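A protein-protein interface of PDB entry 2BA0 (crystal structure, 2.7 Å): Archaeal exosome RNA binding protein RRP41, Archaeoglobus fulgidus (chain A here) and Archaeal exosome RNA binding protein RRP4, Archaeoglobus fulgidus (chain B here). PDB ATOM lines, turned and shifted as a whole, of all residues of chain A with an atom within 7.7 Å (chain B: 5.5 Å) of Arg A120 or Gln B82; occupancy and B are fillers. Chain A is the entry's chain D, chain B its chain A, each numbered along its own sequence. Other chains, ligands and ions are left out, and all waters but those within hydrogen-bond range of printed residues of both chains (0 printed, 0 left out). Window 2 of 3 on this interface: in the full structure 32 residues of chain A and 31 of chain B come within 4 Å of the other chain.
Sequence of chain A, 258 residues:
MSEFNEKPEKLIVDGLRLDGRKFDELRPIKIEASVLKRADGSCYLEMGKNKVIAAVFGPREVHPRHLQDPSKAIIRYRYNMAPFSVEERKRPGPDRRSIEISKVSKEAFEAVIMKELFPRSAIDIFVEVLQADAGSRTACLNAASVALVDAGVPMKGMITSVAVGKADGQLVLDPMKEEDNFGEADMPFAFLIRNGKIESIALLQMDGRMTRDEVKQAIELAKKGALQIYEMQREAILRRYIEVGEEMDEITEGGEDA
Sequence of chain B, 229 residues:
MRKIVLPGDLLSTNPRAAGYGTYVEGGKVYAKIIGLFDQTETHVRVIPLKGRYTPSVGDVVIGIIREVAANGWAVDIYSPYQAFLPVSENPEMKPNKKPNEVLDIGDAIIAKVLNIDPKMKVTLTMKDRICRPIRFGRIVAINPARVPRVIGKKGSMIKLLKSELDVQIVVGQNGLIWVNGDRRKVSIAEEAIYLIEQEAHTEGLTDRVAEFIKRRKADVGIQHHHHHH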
ATOM      1  N   PRO A  59      21.879  13.999 -14.901  1.00  0.00           N
ATOM      2  CA  PRO A  59      21.879  13.230 -13.655  1.00  0.00           C
ATOM      3  C   PRO A  59      22.799  11.999 -13.705  1.00  0.00           C
ATOM      4  O   PRO A  59      22.520  10.991 -14.361  1.00  0.00           O
ATOM      5  CB  PRO A  59      20.393  12.910 -13.462  1.00  0.00           C
ATOM      6  CG  PRO A  59      19.844  12.960 -14.821  1.00  0.00           C
ATOM      7  CD  PRO A  59      20.502  14.179 -15.371  1.00  0.00           C
ATOM      8  N   ARG A  60      23.922  12.108 -13.011  1.00  0.00           N
ATOM      9  CA  ARG A  60      24.916  11.036 -12.966  1.00  0.00           C
ATOM     10  C   ARG A  60      25.202  10.654 -11.526  1.00  0.00           C
ATOM     11  O   ARG A  60      24.753  11.332 -10.604  1.00  0.00           O
ATOM     12  CB  ARG A  60      26.214  11.507 -13.622  1.00  0.00           C
ATOM     13  CG  ARG A  60      26.399  13.016 -13.451  1.00  0.00           C
ATOM     14  CD  ARG A  60      27.815  13.518 -13.298  1.00  0.00           C
ATOM     15  NE  ARG A  60      28.693  13.138 -14.392  1.00  0.00           N
ATOM     16  CZ  ARG A  60      29.761  13.851 -14.721  1.00  0.00           C
ATOM     17  NH1 ARG A  60      30.556  13.477 -15.714  1.00  0.00           N
ATOM     18  NH2 ARG A  60      30.010  14.970 -14.059  1.00  0.00           N
ATOM     19  N   GLU A  61      25.968   9.583 -11.340  1.00  0.00           N
ATOM     20  CA  GLU A  61      26.327   9.113 -10.003  1.00  0.00           C
ATOM     21  C   GLU A  61      27.392   9.995  -9.374  1.00  0.00           C
ATOM     22  O   GLU A  61      28.486  10.104  -9.910  1.00  0.00           O
ATOM     23  CB  GLU A  61      26.875   7.685 -10.072  1.00  0.00           C
ATOM     24  CG  GLU A  61      25.873   6.655 -10.585  1.00  0.00           C
ATOM     25  CD  GLU A  61      26.436   5.244 -10.647  1.00  0.00           C
ATOM     26  OE1 GLU A  61      25.694   4.331 -11.087  1.00  0.00           O
ATOM     27  OE2 GLU A  61      27.611   5.055 -10.259  1.00  0.00           O
ATOM     28  N   VAL A  62      27.087  10.634  -8.252  1.00  0.00           N
ATOM     29  CA  VAL A  62      28.088  11.461  -7.578  1.00  0.00           C
ATOM     30  C   VAL A  62      28.967  10.488  -6.785  1.00  0.00           C
ATOM     31  O   VAL A  62      28.581  10.008  -5.729  1.00  0.00           O
ATOM     32  CB  VAL A  62      27.391  12.474  -6.641  1.00  0.00           C
ATOM     33  CG1 VAL A  62      26.331  11.785  -5.878  1.00  0.00           C
ATOM     34  CG2 VAL A  62      28.351  13.045  -5.657  1.00  0.00           C
ATOM     35  N   HIS A  63      30.147  10.179  -7.305  1.00  0.00           N
ATOM     36  CA  HIS A  63      31.041   9.219  -6.650  1.00  0.00           C
ATOM     37  C   HIS A  63      31.666   9.660  -5.314  1.00  0.00           C
ATOM     38  O   HIS A  63      31.874   8.846  -4.381  1.00  0.00           O
ATOM     39  CB  HIS A  63      32.075   8.758  -7.685  1.00  0.00           C
ATOM     40  CG  HIS A  63      31.505   7.768  -8.653  1.00  0.00           C
ATOM     41  ND1 HIS A  63      30.759   6.679  -8.235  1.00  0.00           N
ATOM     42  CD2 HIS A  63      31.539   7.695 -10.009  1.00  0.00           C
ATOM     43  CE1 HIS A  63      30.367   5.985  -9.285  1.00  0.00           C
ATOM     44  NE2 HIS A  63      30.827   6.577 -10.376  1.00  0.00           N
ATOM     45  N   ARG A  65      31.025   9.965  -2.569  1.00  0.00           N
ATOM     46  CA  ARG A  65      29.925   9.652  -1.664  1.00  0.00           C
ATOM     47  C   ARG A  65      29.510  10.579  -0.520  1.00  0.00           C
ATOM     48  O   ARG A  65      28.330  10.597  -0.165  1.00  0.00           O
ATOM     49  CB  ARG A  65      30.156   8.256  -1.094  1.00  0.00           C
ATOM     50  CG  ARG A  65      29.068   7.307  -1.482  1.00  0.00           C
ATOM     51  CD  ARG A  65      29.601   5.922  -1.820  1.00  0.00           C
ATOM     52  NE  ARG A  65      28.543   5.048  -2.336  1.00  0.00           N
ATOM     53  CZ  ARG A  65      28.664   3.733  -2.506  1.00  0.00           C
ATOM     54  NH1 ARG A  65      27.648   3.022  -2.979  1.00  0.00           N
ATOM     55  NH2 ARG A  65      29.802   3.122  -2.197  1.00  0.00           N
ATOM     56  N   LEU A  67      29.376  13.769  -0.571  1.00  0.00           N
ATOM     57  CA  LEU A  67      28.613  14.879  -1.121  1.00  0.00           C
ATOM     58  C   LEU A  67      27.316  14.388  -1.793  1.00  0.00           C
ATOM     59  O   LEU A  67      26.725  15.087  -2.616  1.00  0.00           O
ATOM     60  CB  LEU A  67      29.474  15.647  -2.128  1.00  0.00           C
ATOM     61  N   GLN A  68      26.862  13.201  -1.413  1.00  0.00           N
ATOM     62  CA  GLN A  68      25.660  12.615  -1.989  1.00  0.00           C
ATOM     63  C   GLN A  68      24.407  12.857  -1.143  1.00  0.00           C
ATOM     64  O   GLN A  68      24.304  12.318  -0.044  1.00  0.00           O
ATOM     65  CB  GLN A  68      25.889  11.100  -2.167  1.00  0.00           C
ATOM     66  CG  GLN A  68      24.705  10.326  -2.710  1.00  0.00           C
ATOM     67  CD  GLN A  68      25.021   8.860  -2.947  1.00  0.00           C
ATOM     68  N   ASP A  69      23.479  13.679  -1.640  1.00  0.00           N
ATOM     69  CA  ASP A  69      22.224  13.976  -0.939  1.00  0.00           C
ATOM     70  C   ASP A  69      21.285  12.786  -1.125  1.00  0.00           C
ATOM     71  O   ASP A  69      21.104  12.279  -2.228  1.00  0.00           O
ATOM     72  CB  ASP A  69      21.590  15.246  -1.516  1.00  0.00           C
ATOM     73  CG  ASP A  69      20.333  15.666  -0.784  1.00  0.00           C
ATOM     74  OD1 ASP A  69      19.503  14.791  -0.444  1.00  0.00           O
ATOM     75  OD2 ASP A  69      20.172  16.881  -0.568  1.00  0.00           O
ATOM     76  N   PRO A  70      20.649  12.348  -0.044  1.00  0.00           N
ATOM     77  CA  PRO A  70      19.737  11.202  -0.100  1.00  0.00           C
ATOM     78  C   PRO A  70      18.327  11.479  -0.603  1.00  0.00           C
ATOM     79  O   PRO A  70      17.590  10.548  -0.932  1.00  0.00           O
ATOM     80  CB  PRO A  70      19.738  10.731   1.341  1.00  0.00           C
ATOM     81  CG  PRO A  70      19.739  12.061   2.075  1.00  0.00           C
ATOM     82  CD  PRO A  70      20.809  12.836   1.340  1.00  0.00           C
ATOM     83  N   SER A  71      17.959  12.753  -0.684  1.00  0.00           N
ATOM     84  CA  SER A  71      16.616  13.103  -1.112  1.00  0.00           C
ATOM     85  C   SER A  71      16.486  13.930  -2.391  1.00  0.00           C
ATOM     86  O   SER A  71      15.382  14.120  -2.880  1.00  0.00           O
ATOM     87  CB  SER A  71      15.903  13.838   0.018  1.00  0.00           C
ATOM     88  OG  SER A  71      16.269  15.205   0.035  1.00  0.00           O
ATOM     89  N   LYS A  72      17.587  14.437  -2.927  1.00  0.00           N
ATOM     90  CA  LYS A  72      17.506  15.230  -4.151  1.00  0.00           C
ATOM     91  C   LYS A  72      18.850  15.315  -4.857  1.00  0.00           C
ATOM     92  O   LYS A  72      19.864  14.868  -4.335  1.00  0.00           O
ATOM     93  CB  LYS A  72      17.002  16.641  -3.836  1.00  0.00           C
ATOM     94  CG  LYS A  72      17.874  17.416  -2.861  1.00  0.00           C
ATOM     95  CD  LYS A  72      17.252  18.765  -2.532  1.00  0.00           C
ATOM     96  CE  LYS A  72      17.844  19.355  -1.261  1.00  0.00           C
ATOM     97  NZ  LYS A  72      17.215  20.671  -0.915  1.00  0.00           N
ATOM     98  N   ALA A  73      18.857  15.883  -6.053  1.00  0.00           N
ATOM     99  CA  ALA A  73      20.100  16.006  -6.791  1.00  0.00           C
ATOM    100  C   ALA A  73      20.824  17.269  -6.357  1.00  0.00           C
ATOM    101  O   ALA A  73      20.193  18.216  -5.879  1.00  0.00           O
ATOM    102  CB  ALA A  73      19.815  16.047  -8.273  1.00  0.00           C
ATOM    103  N   ILE A  74      22.147  17.280  -6.491  1.00  0.00           N
ATOM    104  CA  ILE A  74      22.914  18.461  -6.120  1.00  0.00           C
ATOM    105  C   ILE A  74      23.281  19.093  -7.442  1.00  0.00           C
ATOM    106  O   ILE A  74      23.435  18.391  -8.437  1.00  0.00           O
ATOM    107  CB  ILE A  74      24.225  18.130  -5.328  1.00  0.00           C
ATOM    108  CG1 ILE A  74      25.168  17.302  -6.188  1.00  0.00           C
ATOM    109  CG2 ILE A  74      23.904  17.365  -4.037  1.00  0.00           C
ATOM    110  CD1 ILE A  74      26.436  16.930  -5.487  1.00  0.00           C
ATOM    111  N   LYS A 115      15.158  19.220  -8.821  1.00  0.00           N
ATOM    112  CA  LYS A 115      16.098  18.327  -8.146  1.00  0.00           C
ATOM    113  C   LYS A 115      15.513  17.130  -7.390  1.00  0.00           C
ATOM    114  O   LYS A 115      16.189  16.123  -7.192  1.00  0.00           O
ATOM    115  CB  LYS A 115      16.949  19.146  -7.181  1.00  0.00           C
ATOM    116  CG  LYS A 115      17.682  20.300  -7.839  1.00  0.00           C
ATOM    117  CD  LYS A 115      18.227  21.251  -6.799  1.00  0.00           C
ATOM    118  CE  LYS A 115      17.087  21.962  -6.109  1.00  0.00           C
ATOM    119  NZ  LYS A 115      17.587  22.768  -4.992  1.00  0.00           N
ATOM    120  N   LEU A 117      13.586  15.066  -8.374  1.00  0.00           N
ATOM    121  CA  LEU A 117      13.468  13.936  -9.285  1.00  0.00           C
ATOM    122  C   LEU A 117      14.699  13.023  -9.359  1.00  0.00           C
ATOM    123  O   LEU A 117      14.609  11.932  -9.921  1.00  0.00           O
ATOM    124  CB  LEU A 117      13.116  14.434 -10.699  1.00  0.00           C
ATOM    125  CG  LEU A 117      11.717  15.036 -10.906  1.00  0.00           C
ATOM    126  CD1 LEU A 117      11.521  15.405 -12.374  1.00  0.00           C
ATOM    127  CD2 LEU A 117      10.651  14.029 -10.470  1.00  0.00           C
ATOM    128  N   PHE A 118      15.833  13.448  -8.799  1.00  0.00           N
ATOM    129  CA  PHE A 118      17.041  12.629  -8.865  1.00  0.00           C
ATOM    130  C   PHE A 118      17.891  12.514  -7.594  1.00  0.00           C
ATOM    131  O   PHE A 118      18.995  13.058  -7.515  1.00  0.00           O
ATOM    132  CB  PHE A 118      17.929  13.121 -10.002  1.00  0.00           C
ATOM    133  CG  PHE A 118      17.232  13.195 -11.308  1.00  0.00           C
ATOM    134  CD1 PHE A 118      16.683  14.395 -11.749  1.00  0.00           C
ATOM    135  CD2 PHE A 118      17.100  12.062 -12.101  1.00  0.00           C
ATOM    136  CE1 PHE A 118      16.008  14.461 -12.966  1.00  0.00           C
ATOM    137  CE2 PHE A 118      16.430  12.120 -13.314  1.00  0.00           C
ATOM    138  CZ  PHE A 118      15.885  13.321 -13.746  1.00  0.00           C
ATOM    139  N   PRO A 119      17.403  11.770  -6.592  1.00  0.00           N
ATOM    140  CA  PRO A 119      18.170  11.621  -5.353  1.00  0.00           C
ATOM    141  C   PRO A 119      19.509  10.926  -5.605  1.00  0.00           C
ATOM    142  O   PRO A 119      19.634  10.107  -6.526  1.00  0.00           O
ATOM    143  CB  PRO A 119      17.252  10.769  -4.480  1.00  0.00           C
ATOM    144  CG  PRO A 119      15.873  11.025  -5.050  1.00  0.00           C
ATOM    145  CD  PRO A 119      16.137  11.021  -6.520  1.00  0.00           C
ATOM    146  N   ARG A 120      20.505  11.270  -4.790  1.00  0.00           N
ATOM    147  CA  ARG A 120      21.837  10.669  -4.872  1.00  0.00           C
ATOM    148  C   ARG A 120      22.634  10.957  -6.141  1.00  0.00           C
ATOM    149  O   ARG A 120      23.755  10.476  -6.295  1.00  0.00           O
ATOM    150  CB  ARG A 120      21.732   9.148  -4.705  1.00  0.00           C
ATOM    151  CG  ARG A 120      21.078   8.696  -3.405  1.00  0.00           C
ATOM    152  CD  ARG A 120      19.684   8.107  -3.629  1.00  0.00           C
ATOM    153  NE  ARG A 120      18.868   8.205  -2.418  1.00  0.00           N
ATOM    154  CZ  ARG A 120      17.581   7.872  -2.345  1.00  0.00           C
ATOM    155  NH1 ARG A 120      16.941   7.410  -3.419  1.00  0.00           N
ATOM    156  NH2 ARG A 120      16.927   8.011  -1.196  1.00  0.00           N
ATOM    157  N   SER A 121      22.074  11.741  -7.051  1.00  0.00           N
ATOM    158  CA  SER A 121      22.760  12.028  -8.304  1.00  0.00           C
ATOM    159  C   SER A 121      23.230  13.476  -8.377  1.00  0.00           C
ATOM    160  O   SER A 121      22.906  14.293  -7.522  1.00  0.00           O
ATOM    161  CB  SER A 121      21.830  11.711  -9.493  1.00  0.00           C
ATOM    162  N   ALA A 122      24.007  13.782  -9.406  1.00  0.00           N
ATOM    163  CA  ALA A 122      24.499  15.132  -9.594  1.00  0.00           C
ATOM    164  C   ALA A 122      24.266  15.621 -11.026  1.00  0.00           C
ATOM    165  O   ALA A 122      24.233  14.832 -11.978  1.00  0.00           O
ATOM    166  CB  ALA A 122      25.974  15.182  -9.257  1.00  0.00           C
ATOM    167  N   VAL B  75      20.614  -4.503  -9.136  1.00  0.00           N
ATOM    168  CA  VAL B  75      20.797  -4.522 -10.580  1.00  0.00           C
ATOM    169  C   VAL B  75      21.017  -3.119 -11.137  1.00  0.00           C
ATOM    170  O   VAL B  75      20.377  -2.163 -10.688  1.00  0.00           O
ATOM    171  CB  VAL B  75      19.552  -5.148 -11.273  1.00  0.00           C
ATOM    172  CG1 VAL B  75      19.778  -5.264 -12.770  1.00  0.00           C
ATOM    173  CG2 VAL B  75      19.255  -6.511 -10.672  1.00  0.00           C
ATOM    174  N   SER B  79      20.632   3.893 -15.501  1.00  0.00           N
ATOM    175  CA  SER B  79      19.829   5.089 -15.215  1.00  0.00           C
ATOM    176  C   SER B  79      20.173   5.655 -13.846  1.00  0.00           C
ATOM    177  O   SER B  79      20.786   4.981 -13.030  1.00  0.00           O
ATOM    178  CB  SER B  79      18.330   4.767 -15.230  1.00  0.00           C
ATOM    179  N   PRO B  80      19.794   6.916 -13.586  1.00  0.00           N
ATOM    180  CA  PRO B  80      20.076   7.532 -12.289  1.00  0.00           C
ATOM    181  C   PRO B  80      19.250   6.910 -11.167  1.00  0.00           C
ATOM    182  O   PRO B  80      19.443   7.225  -9.999  1.00  0.00           O
ATOM    183  CB  PRO B  80      19.732   9.005 -12.519  1.00  0.00           C
ATOM    184  CG  PRO B  80      18.683   8.953 -13.577  1.00  0.00           C
ATOM    185  CD  PRO B  80      19.243   7.913 -14.521  1.00  0.00           C
ATOM    186  N   TYR B  81      18.313   6.037 -11.520  1.00  0.00           N
ATOM    187  CA  TYR B  81      17.494   5.380 -10.510  1.00  0.00           C
ATOM    188  C   TYR B  81      18.070   4.002 -10.224  1.00  0.00           C
ATOM    189  O   TYR B  81      18.430   3.269 -11.140  1.00  0.00           O
ATOM    190  CB  TYR B  81      16.035   5.253 -10.972  1.00  0.00           C
ATOM    191  CG  TYR B  81      15.324   6.576 -11.156  1.00  0.00           C
ATOM    192  CD1 TYR B  81      15.556   7.367 -12.281  1.00  0.00           C
ATOM    193  CD2 TYR B  81      14.440   7.054 -10.190  1.00  0.00           C
ATOM    194  CE1 TYR B  81      14.922   8.603 -12.442  1.00  0.00           C
ATOM    195  CE2 TYR B  81      13.804   8.290 -10.337  1.00  0.00           C
ATOM    196  CZ  TYR B  81      14.052   9.059 -11.464  1.00  0.00           C
ATOM    197  OH  TYR B  81      13.444  10.285 -11.610  1.00  0.00           O
ATOM    198  N   GLN B  82      18.168   3.660  -8.946  1.00  0.00           N
ATOM    199  CA  GLN B  82      18.697   2.367  -8.526  1.00  0.00           C
ATOM    200  C   GLN B  82      17.609   1.290  -8.613  1.00  0.00           C
ATOM    201  O   GLN B  82      16.422   1.577  -8.450  1.00  0.00           O
ATOM    202  CB  GLN B  82      19.200   2.475  -7.089  1.00  0.00           C
ATOM    203  CG  GLN B  82      20.079   3.696  -6.838  1.00  0.00           C
ATOM    204  CD  GLN B  82      20.070   4.128  -5.374  1.00  0.00           C
ATOM    205  OE1 GLN B  82      20.672   5.143  -5.008  1.00  0.00           O
ATOM    206  NE2 GLN B  82      19.379   3.357  -4.530  1.00  0.00           N
ATOM    207  N   ALA B  83      18.014   0.052  -8.868  1.00  0.00           N
ATOM    208  CA  ALA B  83      17.055  -1.042  -8.971  1.00  0.00           C
ATOM    209  C   ALA B  83      17.486  -2.258  -8.155  1.00  0.00           C
ATOM    210  O   ALA B  83      18.670  -2.451  -7.893  1.00  0.00           O
ATOM    211  CB  ALA B  83      16.861  -1.430 -10.433  1.00  0.00           C
ATOM    212  N   PHE B  84      16.517  -3.078  -7.760  1.00  0.00           N
ATOM    213  CA  PHE B  84      16.785  -4.270  -6.961  1.00  0.00           C
ATOM    214  C   PHE B  84      15.805  -5.387  -7.295  1.00  0.00           C
ATOM    215  O   PHE B  84      14.598  -5.170  -7.377  1.00  0.00           O
ATOM    216  CB  PHE B  84      16.689  -3.924  -5.465  1.00  0.00           C
ATOM    217  CG  PHE B  84      17.011  -5.075  -4.543  1.00  0.00           C
ATOM    218  CD1 PHE B  84      16.058  -6.055  -4.261  1.00  0.00           C
ATOM    219  CD2 PHE B  84      18.272  -5.174  -3.955  1.00  0.00           C
ATOM    220  CE1 PHE B  84      16.361  -7.116  -3.406  1.00  0.00           C
ATOM    221  CE2 PHE B  84      18.585  -6.228  -3.101  1.00  0.00           C
ATOM    222  CZ  PHE B  84      17.630  -7.200  -2.824  1.00  0.00           C
ATOM    223  N   LYS B 119      10.694   7.003  -2.746  1.00  0.00           N
ATOM    224  CA  LYS B 119      12.091   7.293  -2.448  1.00  0.00           C
ATOM    225  C   LYS B 119      12.938   7.132  -3.716  1.00  0.00           C
ATOM    226  O   LYS B 119      14.165   7.297  -3.688  1.00  0.00           O
ATOM    227  CB  LYS B 119      12.578   6.354  -1.341  1.00  0.00           C
ATOM    228  CG  LYS B 119      13.757   6.876  -0.542  1.00  0.00           C
ATOM    229  CD  LYS B 119      13.924   6.087   0.754  1.00  0.00           C
ATOM    230  CE  LYS B 119      15.029   6.667   1.633  1.00  0.00           C
ATOM    231  NZ  LYS B 119      15.097   5.974   2.954  1.00  0.00           N
ATOM    232  N   MET B 120      12.258   6.808  -4.819  1.00  0.00           N
ATOM    233  CA  MET B 120      12.869   6.622  -6.139  1.00  0.00           C
ATOM    234  C   MET B 120      13.579   5.287  -6.396  1.00  0.00           C
ATOM    235  O   MET B 120      14.359   5.173  -7.345  1.00  0.00           O
ATOM    236  CB  MET B 120      13.840   7.766  -6.442  1.00  0.00           C
ATOM    237  CG  MET B 120      13.196   9.135  -6.465  1.00  0.00           C
ATOM    238  SD  MET B 120      11.771   9.194  -7.551  1.00  0.00           S
ATOM    239  CE  MET B 120      11.116  10.782  -7.144  1.00  0.00           C
ATOM    240  N   LYS B 121      13.324   4.284  -5.560  1.00  0.00           N
ATOM    241  CA  LYS B 121      13.936   2.975  -5.759  1.00  0.00           C
ATOM    242  C   LYS B 121      13.083   2.284  -6.802  1.00  0.00           C
ATOM    243  O   LYS B 121      11.899   2.588  -6.945  1.00  0.00           O
ATOM    244  CB  LYS B 121      13.886   2.120  -4.494  1.00  0.00           C
ATOM    245  CG  LYS B 121      14.076   2.845  -3.180  1.00  0.00           C
ATOM    246  CD  LYS B 121      13.996   1.848  -2.025  1.00  0.00           C
ATOM    247  CE  LYS B 121      12.686   1.048  -2.054  1.00  0.00           C
ATOM    248  NZ  LYS B 121      12.693  -0.131  -1.130  1.00  0.00           N
ATOM    249  N   VAL B 122      13.667   1.347  -7.527  1.00  0.00           N
ATOM    250  CA  VAL B 122      12.910   0.624  -8.526  1.00  0.00           C
ATOM    251  C   VAL B 122      12.987  -0.848  -8.166  1.00  0.00           C
ATOM    252  O   VAL B 122      14.071  -1.376  -7.926  1.00  0.00           O
ATOM    253  CB  VAL B 122      13.486   0.853  -9.942  1.00  0.00           C
ATOM    254  CG1 VAL B 122      12.719   0.022 -10.964  1.00  0.00           C
ATOM    255  CG2 VAL B 122      13.413   2.331 -10.299  1.00  0.00           C
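O of Gln B82 sits at hydrogen-bond distance from N of Val B122, at 2.9 Å. The backbone NH (N) of Ala A73 lies within hydrogen-bond range of the backbone carbonyl oxygen (O) of Phe A118 (3.2 Å). The backbone carbonyl oxygen of Asp A69 sits at hydrogen-bond distance from the backbone NH of Arg A120. O of Pro A70 is in hydrogen-bond range of NH2 of Arg A120, at 2.6 Å.
Gln B82 touches just one residue of chain A: Arg A120. Of the printed residues of chain A, Tyr B81 touches Leu A117 and Phe A118. Printed residues of chain A within 4 Å of Met B120: Pro A119. Of the printed residues of chain B, Phe A118 touches Pro B80 (3.8 Å) and Tyr B81 (3.9 Å). Glu A61 touches none of the printed residues of chain B. Val B75 touches none of the printed residues of chain A. The nearest residue of chain A that does not touch Gln B82 is Pro A119 (5.3 Å).
Among the printed residues, merely in contact across the chains: Pro A59 with Pro B80, Phe A118 with Pro B80, Phe A118 with Tyr B81, Pro A119 with Met B120 and Arg A120 with Gln B82.
The backbone carbonyl oxygen of Leu A117 is in hydrogen-bond range of the side-chain hydroxyl of Tyr B81, 2.6 Å away. O of Lys B119 sits at hydrogen-bond distance from NH1 of Arg A120 (2.8 Å).
Of the 11 printed residues of chain B, 5 touch a printed residue of chain A. Along chain B the printed residues that touch a printed residue of chain A span positions 80 to 120. Printed residues of chain A that touch a printed residue of chain B: Pro A59, Leu A117, Phe A118, Pro A119 and Arg A120. Hydrophobic or aromatic side chains of chain A within 4 Å of the printed part of chain B: Phe A118 and Pro A119. Among the printed residues, 7 pairs touch across the chains.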
